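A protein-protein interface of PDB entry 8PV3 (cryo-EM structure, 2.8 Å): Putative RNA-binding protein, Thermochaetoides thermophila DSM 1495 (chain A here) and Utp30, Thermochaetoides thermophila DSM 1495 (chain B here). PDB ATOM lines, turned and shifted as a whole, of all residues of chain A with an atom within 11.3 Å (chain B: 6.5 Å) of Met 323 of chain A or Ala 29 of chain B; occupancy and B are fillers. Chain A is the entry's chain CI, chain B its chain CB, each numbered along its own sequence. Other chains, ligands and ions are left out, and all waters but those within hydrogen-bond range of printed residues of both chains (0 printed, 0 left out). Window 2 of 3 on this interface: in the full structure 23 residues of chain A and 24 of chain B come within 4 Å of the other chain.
The side-chain carboxylate (OE2) of Glu 326 of chain A is in salt-bridge range of the side-chain amino group (NZ) of Lys 321 of chain A, 3.9 Å away.
O of Ala 29 of chain B touches CE of Met 323 of chain A, at 3.8 Å.
His 33 of chain B touches Met 323 of chain A.
CG of Met 323 of chain A touches CD2 of Leu 291 of chain B, 3.6 Å away.
Tyr 325 of chain A touches Ala 26 of chain B (CE1 to CB, 3.8 Å).
O of Glu 326 of chain A touches NZ of Lys 25 of chain B, 3.97 Å away.
Of chain B, only Ala 29, His 33 and Leu 291 come within 4 Å of Met 323 of chain A.
Ala 29 of chain B touches just one residue of chain A: Met 323 (3.8 Å).
Of the printed residues of chain A, Ala 26 of chain B touches Tyr 325 (3.8 Å).
No residue of chain A comes within 4 Å of Leu 30 of chain B.
Of chain A, only Met 323 (3.5 Å) comes within 4 Å of His 33 of chain B.
No residue of chain A comes within 4 Å of Ala 289 of chain B.
Printed residues of chain B within 4 Å of Tyr 325 of chain A: Ala 26 (3.8 Å).
Of the printed residues of chain B, Glu 326 of chain A touches Lys 25.
Printed residues of chain A within 4 Å of Lys 25 of chain B: Glu 326 (3.97 Å).
Printed residues of chain A within 4 Å of Leu 291 of chain B: Met 323.
Ala 317 of chain A touches none of the printed residues of chain B.
The nearest printed residue of chain B that does not touch Glu 326 of chain A is Ala 29 of chain B (7.2 Å).
Of the 13 printed residues of chain A, 3 touch a printed residue of chain B.
Of the 14 printed residues of chain B, 5 touch a printed residue of chain A.
Printed residues of chain B that touch a printed residue of chain A: Lys 25, Ala 26, Ala 29, His 33 and Leu 291.
Hydrophobic or aromatic side chains of chain B within 4 Å of the printed part of chain A: Ala 26, His 33 and Leu 291.
Among the printed residues, 5 pairs touch across the chains.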
ATOM      1  N   ALA A 315     -12.588 -18.623  20.853  1.00  0.00           N
ATOM      2  CA  ALA A 315     -11.225 -18.965  20.466  1.00  0.00           C
ATOM      3  C   ALA A 315     -10.487 -17.744  19.944  1.00  0.00           C
ATOM      4  O   ALA A 315      -9.318 -17.513  20.285  1.00  0.00           O
ATOM      5  CB  ALA A 315     -11.246 -20.076  19.419  1.00  0.00           C
ATOM      6  N   ARG A 316     -11.176 -16.924  19.147  1.00  0.00           N
ATOM      7  CA  ARG A 316     -10.596 -15.658  18.720  1.00  0.00           C
ATOM      8  C   ARG A 316     -10.347 -14.739  19.911  1.00  0.00           C
ATOM      9  O   ARG A 316      -9.432 -13.914  19.883  1.00  0.00           O
ATOM     10  CB  ARG A 316     -11.497 -14.987  17.682  1.00  0.00           C
ATOM     11  CG  ARG A 316     -11.462 -15.680  16.329  1.00  0.00           C
ATOM     12  CD  ARG A 316     -12.264 -14.938  15.271  1.00  0.00           C
ATOM     13  NE  ARG A 316     -13.702 -14.996  15.506  1.00  0.00           N
ATOM     14  CZ  ARG A 316     -14.607 -14.403  14.740  1.00  0.00           C
ATOM     15  NH1 ARG A 316     -14.255 -13.701  13.675  1.00  0.00           N
ATOM     16  NH2 ARG A 316     -15.895 -14.518  15.047  1.00  0.00           N
ATOM     17  N   ALA A 317     -11.130 -14.891  20.986  1.00  0.00           N
ATOM     18  CA  ALA A 317     -10.893 -14.078  22.177  1.00  0.00           C
ATOM     19  C   ALA A 317      -9.604 -14.468  22.903  1.00  0.00           C
ATOM     20  O   ALA A 317      -8.838 -13.583  23.306  1.00  0.00           O
ATOM     21  CB  ALA A 317     -12.090 -14.133  23.130  1.00  0.00           C
ATOM     22  N   GLU A 318      -9.320 -15.770  23.091  1.00  0.00           N
ATOM     23  CA  GLU A 318      -8.012 -16.047  23.710  1.00  0.00           C
ATOM     24  C   GLU A 318      -6.881 -15.829  22.710  1.00  0.00           C
ATOM     25  O   GLU A 318      -5.716 -15.699  23.101  1.00  0.00           O
ATOM     26  CB  GLU A 318      -7.798 -17.428  24.375  1.00  0.00           C
ATOM     27  CG  GLU A 318      -7.708 -18.715  23.543  1.00  0.00           C
ATOM     28  CD  GLU A 318      -9.019 -19.359  23.259  1.00  0.00           C
ATOM     29  OE1 GLU A 318     -10.032 -18.705  23.452  1.00  0.00           O
ATOM     30  OE2 GLU A 318      -9.037 -20.527  22.821  1.00  0.00           O
ATOM     31  N   LYS A 319      -7.194 -15.798  21.413  1.00  0.00           N
ATOM     32  CA  LYS A 319      -6.185 -15.363  20.452  1.00  0.00           C
ATOM     33  C   LYS A 319      -5.878 -13.876  20.606  1.00  0.00           C
ATOM     34  O   LYS A 319      -4.725 -13.455  20.460  1.00  0.00           O
ATOM     35  CB  LYS A 319      -6.630 -15.691  19.029  1.00  0.00           C
ATOM     36  CG  LYS A 319      -5.929 -16.910  18.452  1.00  0.00           C
ATOM     37  CD  LYS A 319      -6.348 -18.185  19.165  1.00  0.00           C
ATOM     38  CE  LYS A 319      -5.685 -19.405  18.550  1.00  0.00           C
ATOM     39  NZ  LYS A 319      -5.975 -20.662  19.298  1.00  0.00           N
ATOM     40  N   LEU A 320      -6.896 -13.064  20.902  1.00  0.00           N
ATOM     41  CA  LEU A 320      -6.666 -11.627  21.025  1.00  0.00           C
ATOM     42  C   LEU A 320      -6.394 -11.207  22.468  1.00  0.00           C
ATOM     43  O   LEU A 320      -6.340 -10.008  22.762  1.00  0.00           O
ATOM     44  CB  LEU A 320      -7.843 -10.840  20.429  1.00  0.00           C
ATOM     45  CG  LEU A 320      -9.295 -10.903  20.923  1.00  0.00           C
ATOM     46  CD1 LEU A 320      -9.591  -9.997  22.109  1.00  0.00           C
ATOM     47  CD2 LEU A 320     -10.235 -10.598  19.763  1.00  0.00           C
ATOM     48  N   LYS A 321      -6.275 -12.164  23.389  1.00  0.00           N
ATOM     49  CA  LYS A 321      -5.722 -11.815  24.698  1.00  0.00           C
ATOM     50  C   LYS A 321      -4.272 -11.355  24.595  1.00  0.00           C
ATOM     51  O   LYS A 321      -3.875 -10.407  25.282  1.00  0.00           O
ATOM     52  CB  LYS A 321      -5.831 -12.985  25.678  1.00  0.00           C
ATOM     53  CG  LYS A 321      -7.245 -13.406  26.094  1.00  0.00           C
ATOM     54  CD  LYS A 321      -7.935 -12.415  27.043  1.00  0.00           C
ATOM     55  CE  LYS A 321      -8.905 -11.471  26.335  1.00  0.00           C
ATOM     56  NZ  LYS A 321      -9.644 -10.609  27.300  1.00  0.00           N
ATOM     57  N   GLU A 322      -3.465 -12.004  23.748  1.00  0.00           N
ATOM     58  CA  GLU A 322      -2.079 -11.576  23.576  1.00  0.00           C
ATOM     59  C   GLU A 322      -1.996 -10.287  22.767  1.00  0.00           C
ATOM     60  O   GLU A 322      -0.969  -9.598  22.780  1.00  0.00           O
ATOM     61  CB  GLU A 322      -1.257 -12.679  22.906  1.00  0.00           C
ATOM     62  CG  GLU A 322      -0.985 -13.885  23.792  1.00  0.00           C
ATOM     63  CD  GLU A 322      -2.078 -14.930  23.710  1.00  0.00           C
ATOM     64  OE1 GLU A 322      -2.973 -14.791  22.851  1.00  0.00           O
ATOM     65  OE2 GLU A 322      -2.050 -15.885  24.515  1.00  0.00           O
ATOM     66  N   MET A 323      -3.070  -9.954  22.050  1.00  0.00           N
ATOM     67  CA  MET A 323      -3.187  -8.728  21.270  1.00  0.00           C
ATOM     68  C   MET A 323      -3.115  -7.461  22.108  1.00  0.00           C
ATOM     69  O   MET A 323      -2.736  -6.412  21.578  1.00  0.00           O
ATOM     70  CB  MET A 323      -4.515  -8.750  20.514  1.00  0.00           C
ATOM     71  CG  MET A 323      -4.579  -7.950  19.256  1.00  0.00           C
ATOM     72  SD  MET A 323      -3.336  -8.414  18.061  1.00  0.00           S
ATOM     73  CE  MET A 323      -2.479  -6.859  18.018  1.00  0.00           C
ATOM     74  N   GLY A 324      -3.468  -7.524  23.388  1.00  0.00           N
ATOM     75  CA  GLY A 324      -3.741  -6.317  24.136  1.00  0.00           C
ATOM     76  C   GLY A 324      -5.051  -5.678  23.748  1.00  0.00           C
ATOM     77  O   GLY A 324      -5.231  -4.472  23.953  1.00  0.00           O
ATOM     78  N   TYR A 325      -5.975  -6.455  23.190  1.00  0.00           N
ATOM     79  CA  TYR A 325      -7.234  -5.964  22.651  1.00  0.00           C
ATOM     80  C   TYR A 325      -8.372  -6.599  23.435  1.00  0.00           C
ATOM     81  O   TYR A 325      -8.213  -7.694  23.983  1.00  0.00           O
ATOM     82  CB  TYR A 325      -7.345  -6.301  21.162  1.00  0.00           C
ATOM     83  CG  TYR A 325      -8.598  -5.803  20.483  1.00  0.00           C
ATOM     84  CD1 TYR A 325      -8.745  -4.462  20.151  1.00  0.00           C
ATOM     85  CD2 TYR A 325      -9.630  -6.676  20.161  1.00  0.00           C
ATOM     86  CE1 TYR A 325      -9.888  -4.003  19.522  1.00  0.00           C
ATOM     87  CE2 TYR A 325     -10.777  -6.226  19.533  1.00  0.00           C
ATOM     88  CZ  TYR A 325     -10.900  -4.889  19.216  1.00  0.00           C
ATOM     89  OH  TYR A 325     -12.038  -4.437  18.590  1.00  0.00           O
ATOM     90  N   GLU A 326      -9.507  -5.907  23.512  1.00  0.00           N
ATOM     91  CA  GLU A 326     -10.679  -6.415  24.217  1.00  0.00           C
ATOM     92  C   GLU A 326     -11.946  -5.958  23.512  1.00  0.00           C
ATOM     93  O   GLU A 326     -12.074  -4.782  23.150  1.00  0.00           O
ATOM     94  CB  GLU A 326     -10.682  -5.953  25.677  1.00  0.00           C
ATOM     95  CG  GLU A 326     -11.855  -6.478  26.502  1.00  0.00           C
ATOM     96  CD  GLU A 326     -11.837  -7.988  26.679  1.00  0.00           C
ATOM     97  OE1 GLU A 326     -10.746  -8.593  26.619  1.00  0.00           O
ATOM     98  OE2 GLU A 326     -12.924  -8.573  26.875  1.00  0.00           O
ATOM     99  N   PHE A 327     -12.878  -6.888  23.318  1.00  0.00           N
ATOM    100  CA  PHE A 327     -14.227  -6.594  22.848  1.00  0.00           C
ATOM    101  C   PHE A 327     -15.249  -7.362  23.666  1.00  0.00           C
ATOM    102  O   PHE A 327     -15.104  -8.571  23.879  1.00  0.00           O
ATOM    103  CB  PHE A 327     -14.384  -6.906  21.360  1.00  0.00           C
ATOM    104  CG  PHE A 327     -15.756  -6.606  20.823  1.00  0.00           C
ATOM    105  CD1 PHE A 327     -16.167  -5.308  20.584  1.00  0.00           C
ATOM    106  CD2 PHE A 327     -16.614  -7.644  20.497  1.00  0.00           C
ATOM    107  CE1 PHE A 327     -17.421  -5.044  20.069  1.00  0.00           C
ATOM    108  CE2 PHE A 327     -17.864  -7.392  19.975  1.00  0.00           C
ATOM    109  CZ  PHE A 327     -18.273  -6.089  19.766  1.00  0.00           C
ATOM    110  N   LEU B  24     -10.498   3.280  16.872  1.00  0.00           N
ATOM    111  CA  LEU B  24      -9.233   3.955  17.164  1.00  0.00           C
ATOM    112  C   LEU B  24      -8.364   3.143  18.127  1.00  0.00           C
ATOM    113  O   LEU B  24      -7.133   3.093  17.971  1.00  0.00           O
ATOM    114  CB  LEU B  24      -9.512   5.377  17.662  1.00  0.00           C
ATOM    115  CG  LEU B  24     -10.322   5.708  18.925  1.00  0.00           C
ATOM    116  CD1 LEU B  24      -9.574   5.670  20.256  1.00  0.00           C
ATOM    117  CD2 LEU B  24     -11.030   7.047  18.740  1.00  0.00           C
ATOM    118  N   LYS B  25      -8.986   2.463  19.099  1.00  0.00           N
ATOM    119  CA  LYS B  25      -8.229   1.556  19.960  1.00  0.00           C
ATOM    120  C   LYS B  25      -7.620   0.410  19.154  1.00  0.00           C
ATOM    121  O   LYS B  25      -6.466   0.018  19.377  1.00  0.00           O
ATOM    122  CB  LYS B  25      -9.133   1.019  21.073  1.00  0.00           C
ATOM    123  CG  LYS B  25      -8.563  -0.175  21.828  1.00  0.00           C
ATOM    124  CD  LYS B  25      -9.507  -0.655  22.922  1.00  0.00           C
ATOM    125  CE  LYS B  25      -8.886  -1.789  23.731  1.00  0.00           C
ATOM    126  NZ  LYS B  25      -9.700  -2.149  24.928  1.00  0.00           N
ATOM    127  N   ALA B  26      -8.381  -0.123  18.195  1.00  0.00           N
ATOM    128  CA  ALA B  26      -7.892  -1.218  17.364  1.00  0.00           C
ATOM    129  C   ALA B  26      -6.743  -0.774  16.468  1.00  0.00           C
ATOM    130  O   ALA B  26      -5.801  -1.540  16.240  1.00  0.00           O
ATOM    131  CB  ALA B  26      -9.038  -1.794  16.533  1.00  0.00           C
ATOM    132  N   CYS B  27      -6.807   0.455  15.937  1.00  0.00           N
ATOM    133  CA  CYS B  27      -5.680   0.967  15.155  1.00  0.00           C
ATOM    134  C   CYS B  27      -4.433   1.139  16.012  1.00  0.00           C
ATOM    135  O   CYS B  27      -3.326   0.819  15.562  1.00  0.00           O
ATOM    136  CB  CYS B  27      -6.010   2.280  14.434  1.00  0.00           C
ATOM    137  SG  CYS B  27      -7.586   2.408  13.588  1.00  0.00           S
ATOM    138  N   LYS B  28      -4.581   1.637  17.250  1.00  0.00           N
ATOM    139  CA  LYS B  28      -3.398   1.720  18.112  1.00  0.00           C
ATOM    140  C   LYS B  28      -2.823   0.339  18.414  1.00  0.00           C
ATOM    141  O   LYS B  28      -1.601   0.151  18.376  1.00  0.00           O
ATOM    142  CB  LYS B  28      -3.678   2.452  19.423  1.00  0.00           C
ATOM    143  CG  LYS B  28      -4.050   3.905  19.290  1.00  0.00           C
ATOM    144  CD  LYS B  28      -4.207   4.508  20.668  1.00  0.00           C
ATOM    145  CE  LYS B  28      -5.428   3.973  21.345  1.00  0.00           C
ATOM    146  NZ  LYS B  28      -6.610   4.428  20.614  1.00  0.00           N
ATOM    147  N   ALA B  29      -3.687  -0.640  18.701  1.00  0.00           N
ATOM    148  CA  ALA B  29      -3.204  -1.983  19.016  1.00  0.00           C
ATOM    149  C   ALA B  29      -2.518  -2.630  17.814  1.00  0.00           C
ATOM    150  O   ALA B  29      -1.440  -3.224  17.951  1.00  0.00           O
ATOM    151  CB  ALA B  29      -4.362  -2.850  19.510  1.00  0.00           C
ATOM    152  N   LEU B  30      -3.108  -2.493  16.625  1.00  0.00           N
ATOM    153  CA  LEU B  30      -2.539  -3.095  15.425  1.00  0.00           C
ATOM    154  C   LEU B  30      -1.230  -2.415  15.036  1.00  0.00           C
ATOM    155  O   LEU B  30      -0.273  -3.081  14.627  1.00  0.00           O
ATOM    156  CB  LEU B  30      -3.572  -3.044  14.288  1.00  0.00           C
ATOM    157  CG  LEU B  30      -3.365  -3.744  12.937  1.00  0.00           C
ATOM    158  CD1 LEU B  30      -4.711  -4.086  12.328  1.00  0.00           C
ATOM    159  CD2 LEU B  30      -2.603  -2.881  11.949  1.00  0.00           C
ATOM    160  N   LEU B  31      -1.164  -1.088  15.178  1.00  0.00           N
ATOM    161  CA  LEU B  31       0.071  -0.369  14.893  1.00  0.00           C
ATOM    162  C   LEU B  31       1.181  -0.752  15.864  1.00  0.00           C
ATOM    163  O   LEU B  31       2.332  -0.967  15.451  1.00  0.00           O
ATOM    164  CB  LEU B  31      -0.196   1.134  14.930  1.00  0.00           C
ATOM    165  CG  LEU B  31      -0.377   1.830  13.577  1.00  0.00           C
ATOM    166  CD1 LEU B  31      -1.589   1.319  12.817  1.00  0.00           C
ATOM    167  CD2 LEU B  31      -0.470   3.331  13.783  1.00  0.00           C
ATOM    168  N   ALA B  32       0.852  -0.862  17.155  1.00  0.00           N
ATOM    169  CA  ALA B  32       1.841  -1.275  18.144  1.00  0.00           C
ATOM    170  C   ALA B  32       2.339  -2.685  17.858  1.00  0.00           C
ATOM    171  O   ALA B  32       3.534  -2.977  18.003  1.00  0.00           O
ATOM    172  CB  ALA B  32       1.243  -1.179  19.547  1.00  0.00           C
ATOM    173  N   HIS B  33       1.431  -3.565  17.420  1.00  0.00           N
ATOM    174  CA  HIS B  33       1.833  -4.906  17.011  1.00  0.00           C
ATOM    175  C   HIS B  33       2.776  -4.853  15.819  1.00  0.00           C
ATOM    176  O   HIS B  33       3.742  -5.619  15.756  1.00  0.00           O
ATOM    177  CB  HIS B  33       0.607  -5.748  16.670  1.00  0.00           C
ATOM    178  CG  HIS B  33       0.905  -7.194  16.401  1.00  0.00           C
ATOM    179  ND1 HIS B  33      -0.017  -8.043  15.829  1.00  0.00           N
ATOM    180  CD2 HIS B  33       1.996  -7.952  16.668  1.00  0.00           C
ATOM    181  CE1 HIS B  33       0.501  -9.254  15.733  1.00  0.00           C
ATOM    182  NE2 HIS B  33       1.722  -9.227  16.233  1.00  0.00           N
ATOM    183  N   ILE B  34       2.506  -3.956  14.864  1.00  0.00           N
ATOM    184  CA  ILE B  34       3.346  -3.859  13.668  1.00  0.00           C
ATOM    185  C   ILE B  34       4.762  -3.414  14.032  1.00  0.00           C
ATOM    186  O   ILE B  34       5.746  -4.012  13.572  1.00  0.00           O
ATOM    187  CB  ILE B  34       2.692  -2.938  12.619  1.00  0.00           C
ATOM    188  CG1 ILE B  34       1.527  -3.674  11.949  1.00  0.00           C
ATOM    189  CG2 ILE B  34       3.704  -2.477  11.570  1.00  0.00           C
ATOM    190  CD1 ILE B  34       0.893  -2.928  10.803  1.00  0.00           C
ATOM    191  N   THR B 288      -0.626  -9.771  10.205  1.00  0.00           N
ATOM    192  CA  THR B 288      -1.176  -9.715  11.548  1.00  0.00           C
ATOM    193  C   THR B 288      -2.510 -10.456  11.601  1.00  0.00           C
ATOM    194  O   THR B 288      -3.062 -10.876  10.581  1.00  0.00           O
ATOM    195  CB  THR B 288      -1.344  -8.266  11.998  1.00  0.00           C
ATOM    196  OG1 THR B 288      -2.523  -7.713  11.399  1.00  0.00           O
ATOM    197  CG2 THR B 288      -0.137  -7.438  11.585  1.00  0.00           C
ATOM    198  N   ALA B 289      -3.036 -10.619  12.809  1.00  0.00           N
ATOM    199  CA  ALA B 289      -4.334 -11.244  13.000  1.00  0.00           C
ATOM    200  C   ALA B 289      -5.449 -10.250  12.685  1.00  0.00           C
ATOM    201  O   ALA B 289      -5.217  -9.060  12.467  1.00  0.00           O
ATOM    202  CB  ALA B 289      -4.472 -11.773  14.426  1.00  0.00           C
ATOM    203  N   LEU B 291      -8.572  -8.126  13.799  1.00  0.00           N
ATOM    204  CA  LEU B 291      -9.155  -7.515  14.979  1.00  0.00           C
ATOM    205  C   LEU B 291     -10.587  -7.130  14.656  1.00  0.00           C
ATOM    206  O   LEU B 291     -10.803  -6.286  13.773  1.00  0.00           O
ATOM    207  CB  LEU B 291      -8.360  -6.284  15.408  1.00  0.00           C
ATOM    208  CG  LEU B 291      -6.834  -6.329  15.330  1.00  0.00           C
ATOM    209  CD1 LEU B 291      -6.253  -5.040  15.881  1.00  0.00           C
ATOM    210  CD2 LEU B 291      -6.276  -7.525  16.074  1.00  0.00           C
